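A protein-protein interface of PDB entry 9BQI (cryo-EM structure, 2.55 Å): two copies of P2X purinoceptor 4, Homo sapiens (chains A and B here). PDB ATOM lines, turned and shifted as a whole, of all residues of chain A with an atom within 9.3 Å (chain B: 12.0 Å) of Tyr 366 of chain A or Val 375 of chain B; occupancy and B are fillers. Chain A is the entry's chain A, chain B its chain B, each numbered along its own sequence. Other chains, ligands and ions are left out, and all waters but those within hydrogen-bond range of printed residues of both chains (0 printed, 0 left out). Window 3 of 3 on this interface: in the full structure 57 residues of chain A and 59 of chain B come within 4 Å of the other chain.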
ATOM      1  N   ARG A  19     -37.948  16.355   3.912  1.00  0.00           N
ATOM      2  CA  ARG A  19     -37.123  16.473   5.105  1.00  0.00           C
ATOM      3  C   ARG A  19     -35.677  16.161   4.736  1.00  0.00           C
ATOM      4  O   ARG A  19     -35.399  15.130   4.114  1.00  0.00           O
ATOM      5  CB  ARG A  19     -37.619  15.517   6.192  1.00  0.00           C
ATOM      6  CG  ARG A  19     -36.925  15.650   7.535  1.00  0.00           C
ATOM      7  CD  ARG A  19     -37.601  16.696   8.398  1.00  0.00           C
ATOM      8  NE  ARG A  19     -36.805  17.058   9.564  1.00  0.00           N
ATOM      9  CZ  ARG A  19     -36.690  16.312  10.654  1.00  0.00           C
ATOM     10  NH1 ARG A  19     -37.291  15.138  10.758  1.00  0.00           N
ATOM     11  NH2 ARG A  19     -35.956  16.759  11.670  1.00  0.00           N
ATOM     12  N   ILE A  20     -34.764  17.048   5.119  1.00  0.00           N
ATOM     13  CA  ILE A  20     -33.372  16.976   4.692  1.00  0.00           C
ATOM     14  C   ILE A  20     -32.491  16.661   5.891  1.00  0.00           C
ATOM     15  O   ILE A  20     -32.824  16.979   7.038  1.00  0.00           O
ATOM     16  CB  ILE A  20     -32.925  18.288   4.014  1.00  0.00           C
ATOM     17  CG1 ILE A  20     -33.860  18.651   2.857  1.00  0.00           C
ATOM     18  CG2 ILE A  20     -31.501  18.175   3.519  1.00  0.00           C
ATOM     19  CD1 ILE A  20     -33.865  17.655   1.721  1.00  0.00           C
ATOM     20  N   VAL A  21     -31.353  16.026   5.615  1.00  0.00           N
ATOM     21  CA  VAL A  21     -30.349  15.700   6.621  1.00  0.00           C
ATOM     22  C   VAL A  21     -29.062  16.416   6.238  1.00  0.00           C
ATOM     23  O   VAL A  21     -28.562  16.244   5.119  1.00  0.00           O
ATOM     24  CB  VAL A  21     -30.117  14.185   6.732  1.00  0.00           C
ATOM     25  CG1 VAL A  21     -29.269  13.867   7.953  1.00  0.00           C
ATOM     26  CG2 VAL A  21     -31.442  13.442   6.794  1.00  0.00           C
ATOM     27  N   LEU A  22     -28.529  17.211   7.161  1.00  0.00           N
ATOM     28  CA  LEU A  22     -27.317  17.986   6.928  1.00  0.00           C
ATOM     29  C   LEU A  22     -26.140  17.282   7.588  1.00  0.00           C
ATOM     30  O   LEU A  22     -26.148  17.055   8.802  1.00  0.00           O
ATOM     31  CB  LEU A  22     -27.466  19.406   7.476  1.00  0.00           C
ATOM     32  CG  LEU A  22     -28.460  20.320   6.758  1.00  0.00           C
ATOM     33  CD1 LEU A  22     -28.472  21.689   7.405  1.00  0.00           C
ATOM     34  CD2 LEU A  22     -28.129  20.435   5.282  1.00  0.00           C
ATOM     35  N   ILE A  23     -25.132  16.942   6.789  1.00  0.00           N
ATOM     36  CA  ILE A  23     -23.926  16.273   7.260  1.00  0.00           C
ATOM     37  C   ILE A  23     -22.754  17.226   7.082  1.00  0.00           C
ATOM     38  O   ILE A  23     -22.518  17.731   5.978  1.00  0.00           O
ATOM     39  CB  ILE A  23     -23.683  14.956   6.504  1.00  0.00           C
ATOM     40  CG1 ILE A  23     -24.747  13.924   6.875  1.00  0.00           C
ATOM     41  CG2 ILE A  23     -22.298  14.415   6.811  1.00  0.00           C
ATOM     42  CD1 ILE A  23     -25.069  12.955   5.763  1.00  0.00           C
ATOM     43  N   ARG A  24     -22.023  17.472   8.167  1.00  0.00           N
ATOM     44  CA  ARG A  24     -20.842  18.333   8.128  1.00  0.00           C
ATOM     45  C   ARG A  24     -19.649  17.493   7.695  1.00  0.00           C
ATOM     46  O   ARG A  24     -19.042  16.787   8.504  1.00  0.00           O
ATOM     47  CB  ARG A  24     -20.602  18.978   9.488  1.00  0.00           C
ATOM     48  CG  ARG A  24     -21.770  19.800  10.002  1.00  0.00           C
ATOM     49  CD  ARG A  24     -21.320  20.795  11.063  1.00  0.00           C
ATOM     50  NE  ARG A  24     -22.318  20.976  12.110  1.00  0.00           N
ATOM     51  CZ  ARG A  24     -23.534  21.469  11.912  1.00  0.00           C
ATOM     52  NH1 ARG A  24     -23.938  21.858  10.714  1.00  0.00           N
ATOM     53  NH2 ARG A  24     -24.365  21.578  12.946  1.00  0.00           N
ATOM     54  N   SER A  25     -19.307  17.567   6.412  1.00  0.00           N
ATOM     55  CA  SER A  25     -18.168  16.840   5.860  1.00  0.00           C
ATOM     56  C   SER A  25     -17.526  17.704   4.789  1.00  0.00           C
ATOM     57  O   SER A  25     -18.158  18.008   3.773  1.00  0.00           O
ATOM     58  CB  SER A  25     -18.600  15.491   5.280  1.00  0.00           C
ATOM     59  OG  SER A  25     -17.517  14.847   4.634  1.00  0.00           O
ATOM     60  N   VAL A 357     -20.923   8.568   1.021  1.00  0.00           N
ATOM     61  CA  VAL A 357     -21.182   8.743   2.445  1.00  0.00           C
ATOM     62  C   VAL A 357     -21.595   7.427   3.089  1.00  0.00           C
ATOM     63  O   VAL A 357     -21.197   7.124   4.221  1.00  0.00           O
ATOM     64  CB  VAL A 357     -22.250   9.834   2.651  1.00  0.00           C
ATOM     65  CG1 VAL A 357     -22.792   9.789   4.067  1.00  0.00           C
ATOM     66  CG2 VAL A 357     -21.677  11.204   2.342  1.00  0.00           C
ATOM     67  N   LEU A 358     -22.399   6.628   2.390  1.00  0.00           N
ATOM     68  CA  LEU A 358     -22.972   5.428   2.983  1.00  0.00           C
ATOM     69  C   LEU A 358     -22.106   4.189   2.812  1.00  0.00           C
ATOM     70  O   LEU A 358     -22.355   3.186   3.490  1.00  0.00           O
ATOM     71  CB  LEU A 358     -24.352   5.154   2.375  1.00  0.00           C
ATOM     72  CG  LEU A 358     -25.403   6.249   2.571  1.00  0.00           C
ATOM     73  CD1 LEU A 358     -26.582   6.020   1.642  1.00  0.00           C
ATOM     74  CD2 LEU A 358     -25.863   6.309   4.017  1.00  0.00           C
ATOM     75  N   MET A 361     -16.999   5.430   4.301  1.00  0.00           N
ATOM     76  CA  MET A 361     -16.619   6.171   5.495  1.00  0.00           C
ATOM     77  C   MET A 361     -16.633   5.242   6.700  1.00  0.00           C
ATOM     78  O   MET A 361     -17.207   4.150   6.664  1.00  0.00           O
ATOM     79  CB  MET A 361     -17.545   7.361   5.760  1.00  0.00           C
ATOM     80  CG  MET A 361     -17.459   8.471   4.742  1.00  0.00           C
ATOM     81  SD  MET A 361     -18.593   9.804   5.155  1.00  0.00           S
ATOM     82  CE  MET A 361     -18.346  10.894   3.764  1.00  0.00           C
ATOM     83  N   LYS A 362     -15.980   5.695   7.772  1.00  0.00           N
ATOM     84  CA  LYS A 362     -16.001   4.957   9.030  1.00  0.00           C
ATOM     85  C   LYS A 362     -17.322   5.147   9.766  1.00  0.00           C
ATOM     86  O   LYS A 362     -17.792   4.233  10.451  1.00  0.00           O
ATOM     87  CB  LYS A 362     -14.832   5.392   9.912  1.00  0.00           C
ATOM     88  N   LYS A 363     -17.948   6.320   9.617  1.00  0.00           N
ATOM     89  CA  LYS A 363     -19.262   6.620  10.249  1.00  0.00           C
ATOM     90  C   LYS A 363     -20.374   6.333   9.239  1.00  0.00           C
ATOM     91  O   LYS A 363     -21.415   6.991   9.311  1.00  0.00           O
ATOM     92  CB  LYS A 363     -19.332   8.080  10.699  1.00  0.00           C
ATOM     93  CG  LYS A 363     -18.362   8.488  11.796  1.00  0.00           C
ATOM     94  CD  LYS A 363     -18.498   9.943  12.194  1.00  0.00           C
ATOM     95  CE  LYS A 363     -19.908  10.329  12.585  1.00  0.00           C
ATOM     96  NZ  LYS A 363     -19.976  11.718  13.094  1.00  0.00           N
ATOM     97  N   ARG A 364     -20.156   5.384   8.333  1.00  0.00           N
ATOM     98  CA  ARG A 364     -21.148   5.080   7.271  1.00  0.00           C
ATOM     99  C   ARG A 364     -22.374   4.410   7.889  1.00  0.00           C
ATOM    100  O   ARG A 364     -23.398   4.332   7.187  1.00  0.00           O
ATOM    101  CB  ARG A 364     -20.504   4.175   6.220  1.00  0.00           C
ATOM    102  CG  ARG A 364     -19.989   2.852   6.761  1.00  0.00           C
ATOM    103  CD  ARG A 364     -19.225   2.108   5.685  1.00  0.00           C
ATOM    104  NE  ARG A 364     -18.132   1.332   6.250  1.00  0.00           N
ATOM    105  CZ  ARG A 364     -17.256   0.639   5.535  1.00  0.00           C
ATOM    106  NH1 ARG A 364     -17.447   0.469   4.240  1.00  0.00           N
ATOM    107  NH2 ARG A 364     -16.189   0.122   6.119  1.00  0.00           N
ATOM    108  N   LEU A 365     -22.279   3.940   9.135  1.00  0.00           N
ATOM    109  CA  LEU A 365     -23.392   3.261   9.848  1.00  0.00           C
ATOM    110  C   LEU A 365     -24.169   4.310  10.642  1.00  0.00           C
ATOM    111  O   LEU A 365     -25.356   4.055  10.901  1.00  0.00           O
ATOM    112  CB  LEU A 365     -22.798   2.177  10.750  1.00  0.00           C
ATOM    113  CG  LEU A 365     -21.810   1.229  10.074  1.00  0.00           C
ATOM    114  CD1 LEU A 365     -21.399   0.114  11.020  1.00  0.00           C
ATOM    115  CD2 LEU A 365     -22.394   0.652   8.797  1.00  0.00           C
ATOM    116  N   TYR A 366     -23.541   5.420  11.043  1.00  0.00           N
ATOM    117  CA  TYR A 366     -24.251   6.522  11.686  1.00  0.00           C
ATOM    118  C   TYR A 366     -25.115   7.272  10.680  1.00  0.00           C
ATOM    119  O   TYR A 366     -26.286   7.574  10.944  1.00  0.00           O
ATOM    120  CB  TYR A 366     -23.237   7.463  12.342  1.00  0.00           C
ATOM    121  CG  TYR A 366     -23.835   8.536  13.221  1.00  0.00           C
ATOM    122  CD1 TYR A 366     -24.798   8.233  14.171  1.00  0.00           C
ATOM    123  CD2 TYR A 366     -23.422   9.857  13.106  1.00  0.00           C
ATOM    124  CE1 TYR A 366     -25.338   9.214  14.979  1.00  0.00           C
ATOM    125  CE2 TYR A 366     -23.955  10.845  13.908  1.00  0.00           C
ATOM    126  CZ  TYR A 366     -24.913  10.518  14.844  1.00  0.00           C
ATOM    127  OH  TYR A 366     -25.448  11.501  15.643  1.00  0.00           O
ATOM    128  N   TYR A 367     -24.554   7.566   9.505  1.00  0.00           N
ATOM    129  CA  TYR A 367     -25.309   8.273   8.478  1.00  0.00           C
ATOM    130  C   TYR A 367     -26.418   7.407   7.896  1.00  0.00           C
ATOM    131  O   TYR A 367     -27.473   7.926   7.523  1.00  0.00           O
ATOM    132  CB  TYR A 367     -24.365   8.747   7.375  1.00  0.00           C
ATOM    133  CG  TYR A 367     -23.209   9.579   7.883  1.00  0.00           C
ATOM    134  CD1 TYR A 367     -23.390  10.510   8.896  1.00  0.00           C
ATOM    135  CD2 TYR A 367     -21.936   9.432   7.350  1.00  0.00           C
ATOM    136  CE1 TYR A 367     -22.338  11.272   9.359  1.00  0.00           C
ATOM    137  CE2 TYR A 367     -20.878  10.189   7.808  1.00  0.00           C
ATOM    138  CZ  TYR A 367     -21.084  11.107   8.813  1.00  0.00           C
ATOM    139  OH  TYR A 367     -20.033  11.865   9.272  1.00  0.00           O
ATOM    140  N   ARG A 368     -26.199   6.094   7.797  1.00  0.00           N
ATOM    141  CA  ARG A 368     -27.264   5.200   7.358  1.00  0.00           C
ATOM    142  C   ARG A 368     -28.422   5.219   8.346  1.00  0.00           C
ATOM    143  O   ARG A 368     -29.592   5.260   7.947  1.00  0.00           O
ATOM    144  CB  ARG A 368     -26.706   3.783   7.181  1.00  0.00           C
ATOM    145  CG  ARG A 368     -27.728   2.632   7.221  1.00  0.00           C
ATOM    146  CD  ARG A 368     -28.195   2.227   5.830  1.00  0.00           C
ATOM    147  NE  ARG A 368     -27.089   1.890   4.943  1.00  0.00           N
ATOM    148  CZ  ARG A 368     -27.230   1.534   3.674  1.00  0.00           C
ATOM    149  NH1 ARG A 368     -28.423   1.464   3.103  1.00  0.00           N
ATOM    150  NH2 ARG A 368     -26.149   1.241   2.958  1.00  0.00           N
ATOM    151  N   GLU A 369     -28.114   5.186   9.643  1.00  0.00           N
ATOM    152  CA  GLU A 369     -29.162   5.239  10.656  1.00  0.00           C
ATOM    153  C   GLU A 369     -29.897   6.574  10.611  1.00  0.00           C
ATOM    154  O   GLU A 369     -31.120   6.621  10.778  1.00  0.00           O
ATOM    155  CB  GLU A 369     -28.555   4.990  12.040  1.00  0.00           C
ATOM    156  CG  GLU A 369     -29.410   5.430  13.230  1.00  0.00           C
ATOM    157  CD  GLU A 369     -28.622   5.467  14.524  1.00  0.00           C
ATOM    158  OE1 GLU A 369     -27.722   4.619  14.699  1.00  0.00           O
ATOM    159  OE2 GLU A 369     -28.904   6.343  15.368  1.00  0.00           O
ATOM    160  N   LYS A 370     -29.164   7.667  10.398  1.00  0.00           N
ATOM    161  CA  LYS A 370     -29.791   8.986  10.384  1.00  0.00           C
ATOM    162  C   LYS A 370     -30.668   9.178   9.149  1.00  0.00           C
ATOM    163  O   LYS A 370     -31.783   9.703   9.249  1.00  0.00           O
ATOM    164  CB  LYS A 370     -28.714  10.071  10.444  1.00  0.00           C
ATOM    165  CG  LYS A 370     -28.070  10.301  11.816  1.00  0.00           C
ATOM    166  CD  LYS A 370     -29.063  10.279  12.971  1.00  0.00           C
ATOM    167  CE  LYS A 370     -28.693  11.298  14.037  1.00  0.00           C
ATOM    168  NZ  LYS A 370     -29.634  11.268  15.190  1.00  0.00           N
ATOM    169  N   LYS A 371     -30.182   8.766   7.977  1.00  0.00           N
ATOM    170  CA  LYS A 371     -30.885   9.051   6.731  1.00  0.00           C
ATOM    171  C   LYS A 371     -32.112   8.163   6.557  1.00  0.00           C
ATOM    172  O   LYS A 371     -33.176   8.642   6.146  1.00  0.00           O
ATOM    173  CB  LYS A 371     -29.929   8.877   5.550  1.00  0.00           C
ATOM    174  CG  LYS A 371     -30.606   8.825   4.190  1.00  0.00           C
ATOM    175  CD  LYS A 371     -29.583   8.907   3.071  1.00  0.00           C
ATOM    176  CE  LYS A 371     -30.218   8.684   1.710  1.00  0.00           C
ATOM    177  NZ  LYS A 371     -31.125   9.796   1.328  1.00  0.00           N
ATOM    178  N   TYR A 372     -31.987   6.874   6.858  1.00  0.00           N
ATOM    179  CA  TYR A 372     -33.048   5.905   6.613  1.00  0.00           C
ATOM    180  C   TYR A 372     -33.787   5.606   7.908  1.00  0.00           C
ATOM    181  O   TYR A 372     -33.164   5.279   8.922  1.00  0.00           O
ATOM    182  CB  TYR A 372     -32.479   4.612   6.027  1.00  0.00           C
ATOM    183  CG  TYR A 372     -32.022   4.739   4.592  1.00  0.00           C
ATOM    184  CD1 TYR A 372     -32.941   4.810   3.557  1.00  0.00           C
ATOM    185  CD2 TYR A 372     -30.674   4.783   4.275  1.00  0.00           C
ATOM    186  CE1 TYR A 372     -32.530   4.927   2.246  1.00  0.00           C
ATOM    187  CE2 TYR A 372     -30.254   4.899   2.966  1.00  0.00           C
ATOM    188  CZ  TYR A 372     -31.186   4.970   1.957  1.00  0.00           C
ATOM    189  OH  TYR A 372     -30.772   5.086   0.650  1.00  0.00           O
ATOM    190  N   ARG B 368     -37.124  26.268   9.309  1.00  0.00           N
ATOM    191  CA  ARG B 368     -35.754  25.819   9.084  1.00  0.00           C
ATOM    192  C   ARG B 368     -35.393  24.698  10.048  1.00  0.00           C
ATOM    193  O   ARG B 368     -34.772  23.703   9.653  1.00  0.00           O
ATOM    194  CB  ARG B 368     -34.794  27.006   9.226  1.00  0.00           C
ATOM    195  CG  ARG B 368     -33.323  26.667   9.525  1.00  0.00           C
ATOM    196  CD  ARG B 368     -32.476  26.604   8.261  1.00  0.00           C
ATOM    197  NE  ARG B 368     -32.562  27.824   7.468  1.00  0.00           N
ATOM    198  CZ  ARG B 368     -31.944  28.007   6.310  1.00  0.00           C
ATOM    199  NH1 ARG B 368     -31.185  27.065   5.773  1.00  0.00           N
ATOM    200  NH2 ARG B 368     -32.089  29.166   5.673  1.00  0.00           N
ATOM    201  N   GLU B 369     -35.771  24.843  11.318  1.00  0.00           N
ATOM    202  CA  GLU B 369     -35.496  23.798  12.298  1.00  0.00           C
ATOM    203  C   GLU B 369     -36.256  22.521  11.959  1.00  0.00           C
ATOM    204  O   GLU B 369     -35.726  21.416  12.117  1.00  0.00           O
ATOM    205  CB  GLU B 369     -35.856  24.299  13.700  1.00  0.00           C
ATOM    206  CG  GLU B 369     -36.040  23.216  14.765  1.00  0.00           C
ATOM    207  CD  GLU B 369     -36.712  23.745  16.015  1.00  0.00           C
ATOM    208  OE1 GLU B 369     -36.473  24.918  16.371  1.00  0.00           O
ATOM    209  OE2 GLU B 369     -37.481  22.988  16.643  1.00  0.00           O
ATOM    210  N   LYS B 370     -37.503  22.654  11.505  1.00  0.00           N
ATOM    211  CA  LYS B 370     -38.307  21.475  11.201  1.00  0.00           C
ATOM    212  C   LYS B 370     -37.797  20.750   9.957  1.00  0.00           C
ATOM    213  O   LYS B 370     -37.712  19.518   9.942  1.00  0.00           O
ATOM    214  CB  LYS B 370     -39.771  21.883  11.013  1.00  0.00           C
ATOM    215  CG  LYS B 370     -40.553  22.186  12.297  1.00  0.00           C
ATOM    216  CD  LYS B 370     -40.270  21.210  13.433  1.00  0.00           C
ATOM    217  CE  LYS B 370     -41.524  20.928  14.242  1.00  0.00           C
ATOM    218  NZ  LYS B 370     -41.260  20.000  15.376  1.00  0.00           N
ATOM    219  N   LYS B 371     -37.457  21.498   8.905  1.00  0.00           N
ATOM    220  CA  LYS B 371     -37.108  20.882   7.629  1.00  0.00           C
ATOM    221  C   LYS B 371     -35.717  20.261   7.661  1.00  0.00           C
ATOM    222  O   LYS B 371     -35.518  19.148   7.158  1.00  0.00           O
ATOM    223  CB  LYS B 371     -37.202  21.922   6.514  1.00  0.00           C
ATOM    224  CG  LYS B 371     -36.559  21.504   5.202  1.00  0.00           C
ATOM    225  CD  LYS B 371     -36.914  22.474   4.088  1.00  0.00           C
ATOM    226  CE  LYS B 371     -36.145  22.174   2.814  1.00  0.00           C
ATOM    227  NZ  LYS B 371     -36.566  20.890   2.196  1.00  0.00           N
ATOM    228  N   TYR B 372     -34.745  20.957   8.242  1.00  0.00           N
ATOM    229  CA  TYR B 372     -33.352  20.529   8.223  1.00  0.00           C
ATOM    230  C   TYR B 372     -32.988  19.891   9.555  1.00  0.00           C
ATOM    231  O   TYR B 372     -33.216  20.482  10.615  1.00  0.00           O
ATOM    232  CB  TYR B 372     -32.423  21.708   7.938  1.00  0.00           C
ATOM    233  CG  TYR B 372     -32.475  22.198   6.509  1.00  0.00           C
ATOM    234  CD1 TYR B 372     -31.880  21.475   5.487  1.00  0.00           C
ATOM    235  CD2 TYR B 372     -33.115  23.383   6.184  1.00  0.00           C
ATOM    236  CE1 TYR B 372     -31.925  21.916   4.183  1.00  0.00           C
ATOM    237  CE2 TYR B 372     -33.166  23.832   4.881  1.00  0.00           C
ATOM    238  CZ  TYR B 372     -32.569  23.096   3.884  1.00  0.00           C
ATOM    239  OH  TYR B 372     -32.615  23.538   2.584  1.00  0.00           O
ATOM    240  N   LYS B 373     -32.429  18.670   9.494  1.00  0.00           N
ATOM    241  CA  LYS B 373     -32.005  17.883  10.686  1.00  0.00           C
ATOM    242  C   LYS B 373     -30.485  17.733  10.643  1.00  0.00           C
ATOM    243  O   LYS B 373     -30.029  16.986   9.781  1.00  0.00           O
ATOM    244  CB  LYS B 373     -32.700  16.520  10.667  1.00  0.00           C
ATOM    245  CG  LYS B 373     -32.448  15.647  11.887  1.00  0.00           C
ATOM    246  CD  LYS B 373     -32.572  14.167  11.603  1.00  0.00           C
ATOM    247  CE  LYS B 373     -31.491  13.659  10.672  1.00  0.00           C
ATOM    248  NZ  LYS B 373     -31.573  12.192  10.486  1.00  0.00           N
ATOM    249  N   TYR B 374     -29.744  18.268  11.614  1.00  0.00           N
ATOM    250  CA  TYR B 374     -28.289  18.346  11.604  1.00  0.00           C
ATOM    251  C   TYR B 374     -27.696  17.106  12.259  1.00  0.00           C
ATOM    252  O   TYR B 374     -28.117  16.714  13.351  1.00  0.00           O
ATOM    253  CB  TYR B 374     -27.807  19.603  12.333  1.00  0.00           C
ATOM    254  CG  TYR B 374     -28.265  20.904  11.706  1.00  0.00           C
ATOM    255  CD1 TYR B 374     -29.611  21.246  11.666  1.00  0.00           C
ATOM    256  CD2 TYR B 374     -27.351  21.788  11.157  1.00  0.00           C
ATOM    257  CE1 TYR B 374     -30.030  22.431  11.095  1.00  0.00           C
ATOM    258  CE2 TYR B 374     -27.759  22.978  10.584  1.00  0.00           C
ATOM    259  CZ  TYR B 374     -29.101  23.295  10.557  1.00  0.00           C
ATOM    260  OH  TYR B 374     -29.517  24.475   9.988  1.00  0.00           O
ATOM    261  N   VAL B 375     -26.723  16.498  11.589  1.00  0.00           N
ATOM    262  CA  VAL B 375     -26.002  15.343  12.107  1.00  0.00           C
ATOM    263  C   VAL B 375     -24.661  15.858  12.618  1.00  0.00           C
ATOM    264  O   VAL B 375     -23.751  16.144  11.837  1.00  0.00           O
ATOM    265  CB  VAL B 375     -25.825  14.256  11.042  1.00  0.00           C
ATOM    266  CG1 VAL B 375     -25.048  13.078  11.609  1.00  0.00           C
ATOM    267  CG2 VAL B 375     -27.179  13.804  10.515  1.00  0.00           C
ATOM    268  N   GLU B 376     -24.538  15.976  13.936  1.00  0.00           N
ATOM    269  CA  GLU B 376     -23.322  16.500  14.547  1.00  0.00           C
ATOM    270  C   GLU B 376     -22.170  15.513  14.401  1.00  0.00           C
ATOM    271  O   GLU B 376     -21.236  15.745  13.632  1.00  0.00           O
ATOM    272  CB  GLU B 376     -23.560  16.815  16.024  1.00  0.00           C
ATOM    273  CG  GLU B 376     -24.558  17.938  16.263  1.00  0.00           C
ATOM    274  CD  GLU B 376     -24.723  18.267  17.732  1.00  0.00           C
ATOM    275  OE1 GLU B 376     -24.092  17.589  18.571  1.00  0.00           O
ATOM    276  OE2 GLU B 376     -25.480  19.209  18.051  1.00  0.00           O
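The guanidinium group (NE) of Arg 19 of chain A is in hydrogen-bond range of the backbone carbonyl oxygen (O) of Lys 370 of chain B, at 2.6 Å. The backbone carbonyl oxygen (O) of Lys 371 of chain B lies within hydrogen-bond range of the backbone NH (N) of Ile 20 of chain A (3.0 Å). O of Lys 371 of chain B is in hydrogen-bond range of NE of Arg 19 of chain A. N of Leu 22 of chain A lies within hydrogen-bond range of O of Lys 373 of chain B, 3.0 Å away. The side-chain amino group (NZ) of Lys 373 of chain B is in hydrogen-bond range of the backbone carbonyl oxygen (O) of Lys 370 of chain A (2.8 Å). The backbone carbonyl oxygen (O) of Leu 22 of chain A sits at hydrogen-bond distance from the backbone NH (N) of Val 375 of chain B. O of Ile 20 of chain A lies within hydrogen-bond range of N of Lys 373 of chain B.
NH2 of Arg 19 of chain A touches CB of Lys 373 of chain B (3.4 Å). Tyr 372 of chain B touches Ile 20 of chain A. O of Lys 373 of chain B touches CA of Val 21 of chain A (3.4 Å). CG1 of Val 21 of chain A touches CG2 of Val 375 of chain B (3.3 Å). Tyr 372 of chain B touches Leu 22 of chain A. CD1 of Leu 22 of chain A touches CE2 of Tyr 374 of chain B, 3.5 Å away. NH1 of Arg 24 of chain A touches CD2 of Tyr 374 of chain B, 3.4 Å away. Tyr 366 of chain A touches Val 375 of chain B (CE2 to CG1, 3.4 Å). Tyr 367 of chain A touches Val 375 of chain B. Val 375 of chain B touches Lys 370 of chain A.
Of the printed residues of chain B, Tyr 366 of chain A touches Val 375 (3.4 Å). Of chain A, only Val 21 (3.3 Å), Leu 22 (2.9 Å), Tyr 366 (3.4 Å), Tyr 367 (3.96 Å) and Lys 370 (3.8 Å) come within 4 Å of Val 375 of chain B. Of the printed residues of chain B, Leu 22 of chain A touches Tyr 372, Lys 373, Tyr 374 and Val 375. No residue of chain B comes within 4 Å of Lys 363 of chain A. No residue of chain B comes within 4 Å of Leu 365 of chain A. Of the printed residues of chain B, Tyr 367 of chain A touches Val 375 (3.96 Å). No residue of chain B comes within 4 Å of Glu 369 of chain A. Of the printed residues of chain B, Ile 20 of chain A touches Lys 371, Tyr 372 and Lys 373. Printed residues of chain A within 4 Å of Lys 371 of chain B: Arg 19 (3.4 Å) and Ile 20 (3.0 Å). Printed residues of chain A within 4 Å of Tyr 372 of chain B: Ile 20 (3.7 Å) and Leu 22 (3.8 Å). Of the printed residues of chain B, Arg 19 of chain A touches Lys 370 (2.6 Å), Lys 371 (3.4 Å) and Lys 373 (3.4 Å). Val 357 of chain A touches none of the printed residues of chain B. The nearest residue of chain A that does not touch Val 375 of chain B is Arg 24 of chain A (4.3 Å).
Of the 21 printed residues of chain A, 8 touch a printed residue of chain B. Hydrophobic or aromatic side chains of chain A that line the printed part of chain B: Ile 20, Val 21, Leu 22, Tyr 366 and Tyr 367. Hydrophobic or aromatic side chains of chain B within 4 Å of the printed part of chain A: Tyr 372, Tyr 374 and Val 375.
Positions printed for both chains: 368, 369, 370, 371 and 372. Of the 17 pairs that touch across the chains among the printed residues, none has its exchanged pair printed and touching as well.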
